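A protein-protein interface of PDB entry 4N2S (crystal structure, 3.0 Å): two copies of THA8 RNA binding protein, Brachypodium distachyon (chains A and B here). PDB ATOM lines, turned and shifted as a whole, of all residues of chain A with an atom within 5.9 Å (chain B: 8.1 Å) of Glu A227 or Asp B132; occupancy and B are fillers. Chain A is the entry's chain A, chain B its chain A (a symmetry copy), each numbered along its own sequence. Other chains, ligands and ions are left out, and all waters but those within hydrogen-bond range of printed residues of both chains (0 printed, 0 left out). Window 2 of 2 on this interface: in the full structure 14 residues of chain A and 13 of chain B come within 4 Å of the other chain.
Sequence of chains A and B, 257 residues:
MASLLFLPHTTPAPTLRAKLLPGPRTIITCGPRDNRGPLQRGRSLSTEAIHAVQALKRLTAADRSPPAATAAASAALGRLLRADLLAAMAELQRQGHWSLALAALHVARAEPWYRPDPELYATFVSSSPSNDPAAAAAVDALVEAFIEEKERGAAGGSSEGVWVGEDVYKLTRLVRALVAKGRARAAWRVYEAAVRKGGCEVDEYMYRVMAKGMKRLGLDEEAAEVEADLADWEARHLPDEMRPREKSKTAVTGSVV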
ATOM      1  N   ALA A 211      20.372 -23.802  -5.096  1.00  0.00           N
ATOM      2  CA  ALA A 211      21.543 -24.656  -4.959  1.00  0.00           C
ATOM      3  C   ALA A 211      22.550 -24.011  -4.017  1.00  0.00           C
ATOM      4  O   ALA A 211      22.922 -24.627  -3.030  1.00  0.00           O
ATOM      5  CB  ALA A 211      22.182 -24.891  -6.310  1.00  0.00           C
ATOM      6  N   LYS A 212      22.979 -22.781  -4.310  1.00  0.00           N
ATOM      7  CA  LYS A 212      23.913 -22.048  -3.449  1.00  0.00           C
ATOM      8  C   LYS A 212      23.316 -21.804  -2.063  1.00  0.00           C
ATOM      9  O   LYS A 212      23.990 -21.942  -1.049  1.00  0.00           O
ATOM     10  CB  LYS A 212      24.297 -20.689  -4.073  1.00  0.00           C
ATOM     11  CG  LYS A 212      24.922 -20.774  -5.453  1.00  0.00           C
ATOM     12  CD  LYS A 212      26.213 -21.604  -5.436  1.00  0.00           C
ATOM     13  CE  LYS A 212      26.496 -22.306  -6.773  1.00  0.00           C
ATOM     14  NZ  LYS A 212      25.481 -23.358  -7.134  1.00  0.00           N
ATOM     15  N   GLU A 222      19.509 -31.235   0.478  1.00  0.00           N
ATOM     16  CA  GLU A 222      18.608 -30.384  -0.285  1.00  0.00           C
ATOM     17  C   GLU A 222      19.330 -29.815  -1.504  1.00  0.00           C
ATOM     18  O   GLU A 222      18.823 -29.865  -2.627  1.00  0.00           O
ATOM     19  CB  GLU A 222      18.099 -29.238   0.589  1.00  0.00           C
ATOM     20  CG  GLU A 222      17.034 -29.636   1.613  1.00  0.00           C
ATOM     21  CD  GLU A 222      17.550 -30.585   2.686  1.00  0.00           C
ATOM     22  OE1 GLU A 222      18.719 -30.467   3.123  1.00  0.00           O
ATOM     23  OE2 GLU A 222      16.780 -31.463   3.112  1.00  0.00           O
ATOM     24  N   ALA A 223      20.520 -29.275  -1.261  1.00  0.00           N
ATOM     25  CA  ALA A 223      21.354 -28.699  -2.309  1.00  0.00           C
ATOM     26  C   ALA A 223      21.627 -29.705  -3.425  1.00  0.00           C
ATOM     27  O   ALA A 223      21.591 -29.359  -4.606  1.00  0.00           O
ATOM     28  CB  ALA A 223      22.665 -28.163  -1.716  1.00  0.00           C
ATOM     29  N   ALA A 224      21.892 -30.950  -3.043  1.00  0.00           N
ATOM     30  CA  ALA A 224      22.183 -32.004  -4.008  1.00  0.00           C
ATOM     31  C   ALA A 224      20.975 -32.251  -4.889  1.00  0.00           C
ATOM     32  O   ALA A 224      21.120 -32.562  -6.064  1.00  0.00           O
ATOM     33  CB  ALA A 224      22.583 -33.276  -3.288  1.00  0.00           C
ATOM     34  N   GLU A 225      19.784 -32.111  -4.309  1.00  0.00           N
ATOM     35  CA  GLU A 225      18.545 -32.314  -5.045  1.00  0.00           C
ATOM     36  C   GLU A 225      18.314 -31.224  -6.071  1.00  0.00           C
ATOM     37  O   GLU A 225      17.930 -31.498  -7.213  1.00  0.00           O
ATOM     38  CB  GLU A 225      17.368 -32.387  -4.093  1.00  0.00           C
ATOM     39  CG  GLU A 225      17.465 -33.552  -3.125  1.00  0.00           C
ATOM     40  CD  GLU A 225      16.285 -33.612  -2.174  1.00  0.00           C
ATOM     41  OE1 GLU A 225      15.127 -33.653  -2.670  1.00  0.00           O
ATOM     42  OE2 GLU A 225      16.523 -33.609  -0.933  1.00  0.00           O
ATOM     43  N   VAL A 226      18.558 -29.983  -5.656  1.00  0.00           N
ATOM     44  CA  VAL A 226      18.396 -28.820  -6.531  1.00  0.00           C
ATOM     45  C   VAL A 226      19.335 -28.950  -7.722  1.00  0.00           C
ATOM     46  O   VAL A 226      18.947 -28.661  -8.854  1.00  0.00           O
ATOM     47  CB  VAL A 226      18.693 -27.503  -5.785  1.00  0.00           C
ATOM     48  CG1 VAL A 226      18.716 -26.346  -6.757  1.00  0.00           C
ATOM     49  CG2 VAL A 226      17.658 -27.257  -4.708  1.00  0.00           C
ATOM     50  N   GLU A 227      20.564 -29.395  -7.465  1.00  0.00           N
ATOM     51  CA  GLU A 227      21.537 -29.590  -8.534  1.00  0.00           C
ATOM     52  C   GLU A 227      21.032 -30.670  -9.483  1.00  0.00           C
ATOM     53  O   GLU A 227      21.320 -30.627 -10.674  1.00  0.00           O
ATOM     54  CB  GLU A 227      22.899 -29.996  -7.979  1.00  0.00           C
ATOM     55  CG  GLU A 227      23.536 -28.945  -7.102  1.00  0.00           C
ATOM     56  CD  GLU A 227      24.977 -29.235  -6.760  1.00  0.00           C
ATOM     57  OE1 GLU A 227      25.281 -30.341  -6.288  1.00  0.00           O
ATOM     58  OE2 GLU A 227      25.795 -28.331  -6.939  1.00  0.00           O
ATOM     59  N   ALA A 228      20.289 -31.639  -8.938  1.00  0.00           N
ATOM     60  CA  ALA A 228      19.727 -32.733  -9.712  1.00  0.00           C
ATOM     61  C   ALA A 228      18.605 -32.205 -10.614  1.00  0.00           C
ATOM     62  O   ALA A 228      18.554 -32.523 -11.804  1.00  0.00           O
ATOM     63  CB  ALA A 228      19.186 -33.768  -8.782  1.00  0.00           C
ATOM     64  N   ASP A 229      17.713 -31.393 -10.046  1.00  0.00           N
ATOM     65  CA  ASP A 229      16.622 -30.782 -10.817  1.00  0.00           C
ATOM     66  C   ASP A 229      17.159 -29.946 -11.957  1.00  0.00           C
ATOM     67  O   ASP A 229      16.598 -29.937 -13.058  1.00  0.00           O
ATOM     68  CB  ASP A 229      15.762 -29.885  -9.937  1.00  0.00           C
ATOM     69  CG  ASP A 229      15.374 -30.540  -8.669  1.00  0.00           C
ATOM     70  OD1 ASP A 229      14.936 -31.697  -8.732  1.00  0.00           O
ATOM     71  OD2 ASP A 229      15.502 -29.906  -7.610  1.00  0.00           O
ATOM     72  N   LEU A 230      18.247 -29.222 -11.670  1.00  0.00           N
ATOM     73  CA  LEU A 230      18.898 -28.383 -12.668  1.00  0.00           C
ATOM     74  C   LEU A 230      19.495 -29.285 -13.742  1.00  0.00           C
ATOM     75  O   LEU A 230      19.379 -28.994 -14.934  1.00  0.00           O
ATOM     76  CB  LEU A 230      20.012 -27.543 -12.035  1.00  0.00           C
ATOM     77  CG  LEU A 230      20.845 -26.706 -13.006  1.00  0.00           C
ATOM     78  CD1 LEU A 230      20.000 -25.654 -13.725  1.00  0.00           C
ATOM     79  CD2 LEU A 230      21.922 -26.022 -12.164  1.00  0.00           C
ATOM     80  N   ALA A 231      20.126 -30.381 -13.312  1.00  0.00           N
ATOM     81  CA  ALA A 231      20.750 -31.325 -14.232  1.00  0.00           C
ATOM     82  C   ALA A 231      19.721 -31.799 -15.226  1.00  0.00           C
ATOM     83  O   ALA A 231      19.989 -31.916 -16.431  1.00  0.00           O
ATOM     84  CB  ALA A 231      21.316 -32.500 -13.482  1.00  0.00           C
ATOM     85  N   ASP A 232      18.541 -32.079 -14.689  1.00  0.00           N
ATOM     86  CA  ASP A 232      17.420 -32.531 -15.482  1.00  0.00           C
ATOM     87  C   ASP A 232      16.928 -31.368 -16.363  1.00  0.00           C
ATOM     88  O   ASP A 232      16.482 -31.572 -17.491  1.00  0.00           O
ATOM     89  CB  ASP A 232      16.317 -33.043 -14.565  1.00  0.00           C
ATOM     90  CG  ASP A 232      15.001 -33.249 -15.312  1.00  0.00           C
ATOM     91  OD1 ASP A 232      14.972 -34.083 -16.258  1.00  0.00           O
ATOM     92  OD2 ASP A 232      14.003 -32.568 -14.954  1.00  0.00           O
ATOM     93  N   GLU A 234      18.837 -28.798 -17.486  1.00  0.00           N
ATOM     94  CA  GLU A 234      19.844 -28.567 -18.484  1.00  0.00           C
ATOM     95  C   GLU A 234      19.838 -29.671 -19.490  1.00  0.00           C
ATOM     96  O   GLU A 234      20.409 -29.550 -20.540  1.00  0.00           O
ATOM     97  CB  GLU A 234      21.213 -28.502 -17.834  1.00  0.00           C
ATOM     98  CG  GLU A 234      21.460 -27.281 -17.004  1.00  0.00           C
ATOM     99  CD  GLU A 234      21.686 -26.061 -17.831  1.00  0.00           C
ATOM    100  OE1 GLU A 234      21.883 -26.197 -19.037  1.00  0.00           O
ATOM    101  OE2 GLU A 234      21.671 -24.957 -17.281  1.00  0.00           O
ATOM    102  N   ALA A 235      19.211 -30.776 -19.165  1.00  0.00           N
ATOM    103  CA  ALA A 235      19.222 -31.885 -20.079  1.00  0.00           C
ATOM    104  C   ALA A 235      18.176 -31.626 -21.101  1.00  0.00           C
ATOM    105  O   ALA A 235      18.343 -31.951 -22.249  1.00  0.00           O
ATOM    106  CB  ALA A 235      18.929 -33.124 -19.369  1.00  0.00           C
ATOM    107  N   TRP B  98      23.462 -20.006 -17.867  1.00  0.00           N
ATOM    108  CA  TRP B  98      24.499 -20.638 -18.676  1.00  0.00           C
ATOM    109  C   TRP B  98      24.013 -20.968 -20.077  1.00  0.00           C
ATOM    110  O   TRP B  98      24.724 -20.742 -21.073  1.00  0.00           O
ATOM    111  CB  TRP B  98      25.007 -21.871 -17.939  1.00  0.00           C
ATOM    112  CG  TRP B  98      26.368 -22.286 -18.324  1.00  0.00           C
ATOM    113  CD1 TRP B  98      27.533 -21.570 -18.172  1.00  0.00           C
ATOM    114  CD2 TRP B  98      26.746 -23.536 -18.953  1.00  0.00           C
ATOM    115  NE1 TRP B  98      28.604 -22.281 -18.660  1.00  0.00           N
ATOM    116  CE2 TRP B  98      28.181 -23.479 -19.143  1.00  0.00           C
ATOM    117  CE3 TRP B  98      26.051 -24.662 -19.376  1.00  0.00           C
ATOM    118  CZ2 TRP B  98      28.878 -24.519 -19.719  1.00  0.00           C
ATOM    119  CZ3 TRP B  98      26.757 -25.709 -19.959  1.00  0.00           C
ATOM    120  CH2 TRP B  98      28.140 -25.641 -20.122  1.00  0.00           C
ATOM    121  N   SER B 128      29.964 -23.086 -15.369  1.00  0.00           N
ATOM    122  CA  SER B 128      29.083 -24.209 -15.653  1.00  0.00           C
ATOM    123  C   SER B 128      28.567 -24.823 -14.325  1.00  0.00           C
ATOM    124  O   SER B 128      29.305 -24.843 -13.328  1.00  0.00           O
ATOM    125  CB  SER B 128      29.799 -25.252 -16.516  1.00  0.00           C
ATOM    126  OG  SER B 128      30.747 -25.951 -15.761  1.00  0.00           O
ATOM    127  N   PRO B 129      27.290 -25.313 -14.314  1.00  0.00           N
ATOM    128  CA  PRO B 129      26.660 -25.950 -13.148  1.00  0.00           C
ATOM    129  C   PRO B 129      27.367 -27.238 -12.753  1.00  0.00           C
ATOM    130  O   PRO B 129      27.514 -28.156 -13.569  1.00  0.00           O
ATOM    131  CB  PRO B 129      25.241 -26.244 -13.656  1.00  0.00           C
ATOM    132  CG  PRO B 129      25.005 -25.194 -14.689  1.00  0.00           C
ATOM    133  CD  PRO B 129      26.315 -25.176 -15.415  1.00  0.00           C
ATOM    134  N   SER B 130      27.808 -27.311 -11.507  1.00  0.00           N
ATOM    135  CA  SER B 130      28.488 -28.514 -11.025  1.00  0.00           C
ATOM    136  C   SER B 130      27.513 -29.660 -10.855  1.00  0.00           C
ATOM    137  O   SER B 130      26.300 -29.431 -10.698  1.00  0.00           O
ATOM    138  CB  SER B 130      29.197 -28.232  -9.711  1.00  0.00           C
ATOM    139  OG  SER B 130      30.251 -27.305  -9.926  1.00  0.00           O
ATOM    140  N   ASN B 131      28.047 -30.878 -10.898  1.00  0.00           N
ATOM    141  CA  ASN B 131      27.228 -32.093 -10.726  1.00  0.00           C
ATOM    142  C   ASN B 131      26.139 -32.164 -11.754  1.00  0.00           C
ATOM    143  O   ASN B 131      25.027 -32.593 -11.449  1.00  0.00           O
ATOM    144  CB  ASN B 131      26.597 -32.163  -9.327  1.00  0.00           C
ATOM    145  CG  ASN B 131      27.621 -32.035  -8.228  1.00  0.00           C
ATOM    146  OD1 ASN B 131      28.224 -30.985  -8.044  1.00  0.00           O
ATOM    147  ND2 ASN B 131      27.834 -33.111  -7.506  1.00  0.00           N
ATOM    148  N   ASP B 132      26.475 -31.728 -12.969  1.00  0.00           N
ATOM    149  CA  ASP B 132      25.531 -31.714 -14.094  1.00  0.00           C
ATOM    150  C   ASP B 132      26.071 -32.506 -15.263  1.00  0.00           C
ATOM    151  O   ASP B 132      26.903 -32.000 -16.022  1.00  0.00           O
ATOM    152  CB  ASP B 132      25.272 -30.287 -14.564  1.00  0.00           C
ATOM    153  CG  ASP B 132      23.954 -29.749 -14.093  1.00  0.00           C
ATOM    154  OD1 ASP B 132      23.757 -29.587 -12.841  1.00  0.00           O
ATOM    155  OD2 ASP B 132      23.146 -29.477 -15.018  1.00  0.00           O
ATOM    156  N   PRO B 133      25.607 -33.756 -15.427  1.00  0.00           N
ATOM    157  CA  PRO B 133      26.041 -34.608 -16.528  1.00  0.00           C
ATOM    158  C   PRO B 133      25.824 -33.925 -17.884  1.00  0.00           C
ATOM    159  O   PRO B 133      26.706 -33.979 -18.769  1.00  0.00           O
ATOM    160  CB  PRO B 133      25.151 -35.833 -16.357  1.00  0.00           C
ATOM    161  CG  PRO B 133      25.005 -35.909 -14.875  1.00  0.00           C
ATOM    162  CD  PRO B 133      24.717 -34.488 -14.518  1.00  0.00           C
ATOM    163  N   ALA B 134      24.661 -33.281 -18.030  1.00  0.00           N
ATOM    164  CA  ALA B 134      24.348 -32.569 -19.271  1.00  0.00           C
ATOM    165  C   ALA B 134      25.414 -31.483 -19.541  1.00  0.00           C
ATOM    166  O   ALA B 134      26.001 -31.395 -20.628  1.00  0.00           O
ATOM    167  CB  ALA B 134      22.947 -31.977 -19.204  1.00  0.00           C
ATOM    168  N   ALA B 135      25.663 -30.672 -18.517  1.00  0.00           N
ATOM    169  CA  ALA B 135      26.618 -29.578 -18.600  1.00  0.00           C
ATOM    170  C   ALA B 135      28.030 -30.107 -18.814  1.00  0.00           C
ATOM    171  O   ALA B 135      28.789 -29.540 -19.601  1.00  0.00           O
ATOM    172  CB  ALA B 135      26.561 -28.734 -17.337  1.00  0.00           C
ATOM    173  N   ALA B 136      28.375 -31.187 -18.113  1.00  0.00           N
ATOM    174  CA  ALA B 136      29.698 -31.801 -18.244  1.00  0.00           C
ATOM    175  C   ALA B 136      29.999 -32.095 -19.707  1.00  0.00           C
ATOM    176  O   ALA B 136      31.107 -31.828 -20.177  1.00  0.00           O
ATOM    177  CB  ALA B 136      29.761 -33.068 -17.453  1.00  0.00           C
ATOM    178  N   ALA B 137      29.009 -32.639 -20.418  1.00  0.00           N
ATOM    179  CA  ALA B 137      29.165 -32.944 -21.828  1.00  0.00           C
ATOM    180  C   ALA B 137      29.411 -31.654 -22.667  1.00  0.00           C
ATOM    181  O   ALA B 137      30.330 -31.578 -23.505  1.00  0.00           O
ATOM    182  CB  ALA B 137      27.933 -33.671 -22.314  1.00  0.00           C
ATOM    183  N   ALA B 138      28.566 -30.654 -22.426  1.00  0.00           N
ATOM    184  CA  ALA B 138      28.657 -29.379 -23.110  1.00  0.00           C
ATOM    185  C   ALA B 138      30.048 -28.787 -22.945  1.00  0.00           C
ATOM    186  O   ALA B 138      30.591 -28.202 -23.889  1.00  0.00           O
ATOM    187  CB  ALA B 138      27.602 -28.423 -22.569  1.00  0.00           C
ATOM    188  N   VAL B 139      30.616 -28.939 -21.742  1.00  0.00           N
ATOM    189  CA  VAL B 139      31.950 -28.423 -21.426  1.00  0.00           C
ATOM    190  C   VAL B 139      32.959 -29.096 -22.346  1.00  0.00           C
ATOM    191  O   VAL B 139      33.828 -28.447 -22.919  1.00  0.00           O
ATOM    192  CB  VAL B 139      32.349 -28.703 -19.968  1.00  0.00           C
ATOM    193  CG1 VAL B 139      33.792 -28.293 -19.710  1.00  0.00           C
ATOM    194  CG2 VAL B 139      31.427 -27.946 -19.025  1.00  0.00           C
ATOM    195  N   LYS B 181      36.500 -28.304 -12.648  1.00  0.00           N
ATOM    196  CA  LYS B 181      35.218 -28.943 -12.889  1.00  0.00           C
ATOM    197  C   LYS B 181      35.407 -30.454 -13.041  1.00  0.00           C
ATOM    198  O   LYS B 181      34.446 -31.194 -13.198  1.00  0.00           O
ATOM    199  CB  LYS B 181      34.583 -28.362 -14.147  1.00  0.00           C
ATOM    200  CG  LYS B 181      34.245 -26.892 -14.014  1.00  0.00           C
ATOM    201  CD  LYS B 181      33.256 -26.678 -12.869  1.00  0.00           C
ATOM    202  CE  LYS B 181      32.771 -25.246 -12.801  1.00  0.00           C
ATOM    203  NZ  LYS B 181      31.578 -25.177 -11.916  1.00  0.00           N
ATOM    204  N   ARG B 183      37.059 -32.107 -15.587  1.00  0.00           N
ATOM    205  CA  ARG B 183      37.000 -32.621 -16.950  1.00  0.00           C
ATOM    206  C   ARG B 183      38.401 -33.049 -17.407  1.00  0.00           C
ATOM    207  O   ARG B 183      38.957 -32.503 -18.366  1.00  0.00           O
ATOM    208  CB  ARG B 183      36.415 -31.574 -17.903  1.00  0.00           C
ATOM    209  CG  ARG B 183      35.131 -30.922 -17.411  1.00  0.00           C
ATOM    210  CD  ARG B 183      34.176 -31.945 -16.867  1.00  0.00           C
ATOM    211  NE  ARG B 183      33.956 -33.002 -17.850  1.00  0.00           N
ATOM    212  CZ  ARG B 183      33.465 -34.200 -17.546  1.00  0.00           C
ATOM    213  NH1 ARG B 183      33.161 -34.489 -16.297  1.00  0.00           N
ATOM    214  NH2 ARG B 183      33.289 -35.110 -18.475  1.00  0.00           N
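Along chain A the printed residues that touch a printed residue of chain B span positions 227 to 235. Of the 15 printed residues of chain B, 5 touch a printed residue of chain A. Hydrophobic or aromatic side chains of chain B within 4 Å of the printed part of chain A: Pro B129 and Ala B134. Among the printed residues, no Asp or Glu carboxylate lies within 4 Å of a Lys or Arg side-chain nitrogen of the other chain.
OE1 of Glu A227 sits close to OD1 of Asn B131, at 3.5 Å. O of Glu A227 lies close to OD1 of Asp B132, at 3.4 Å.
Glu A227 touches just these residues of chain B: Ser B130 (3.9 Å), Asn B131 (3.5 Å) and Asp B132 (3.4 Å). No residue of chain B comes within 4 Å of Ala A228. Of the printed residues of chain B, Leu A230 touches Pro B129 and Asp B132. Of the printed residues of chain B, Ala A231 touches Asp B132 (3.1 Å). Ser B128 touches none of the printed residues of chain A. Asp B132 touches four residues of chain A. Pro B133 touches none of the printed residues of chain A. The nearest residue of chain A that does not touch Asp B132 is Asp A232 (5.3 Å). The nearest printed residue of chain B that does not touch Ala A235 is Asp B132 (5.9 Å).
Among the printed residues, merely in contact across the chains: Glu A227 with Ser B130 (3.9 Å), Leu A230 with Pro B129 (3.6 Å), Leu A230 with Asp B132 (3.8 Å), Ala A231 with Asp B132 (3.1 Å), Glu A234 with Asp B132 (3.4 Å), Glu A234 with Ala B134 (3.8 Å) and Ala A235 with Ala B134 (3.8 Å).
No position is printed for both chains. Of the 9 pairs that touch across the chains among the printed residues, none has its exchanged pair printed and touching as well.
OG of Ser B130 is in hydrogen-bond range of NZ of Lys B181.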
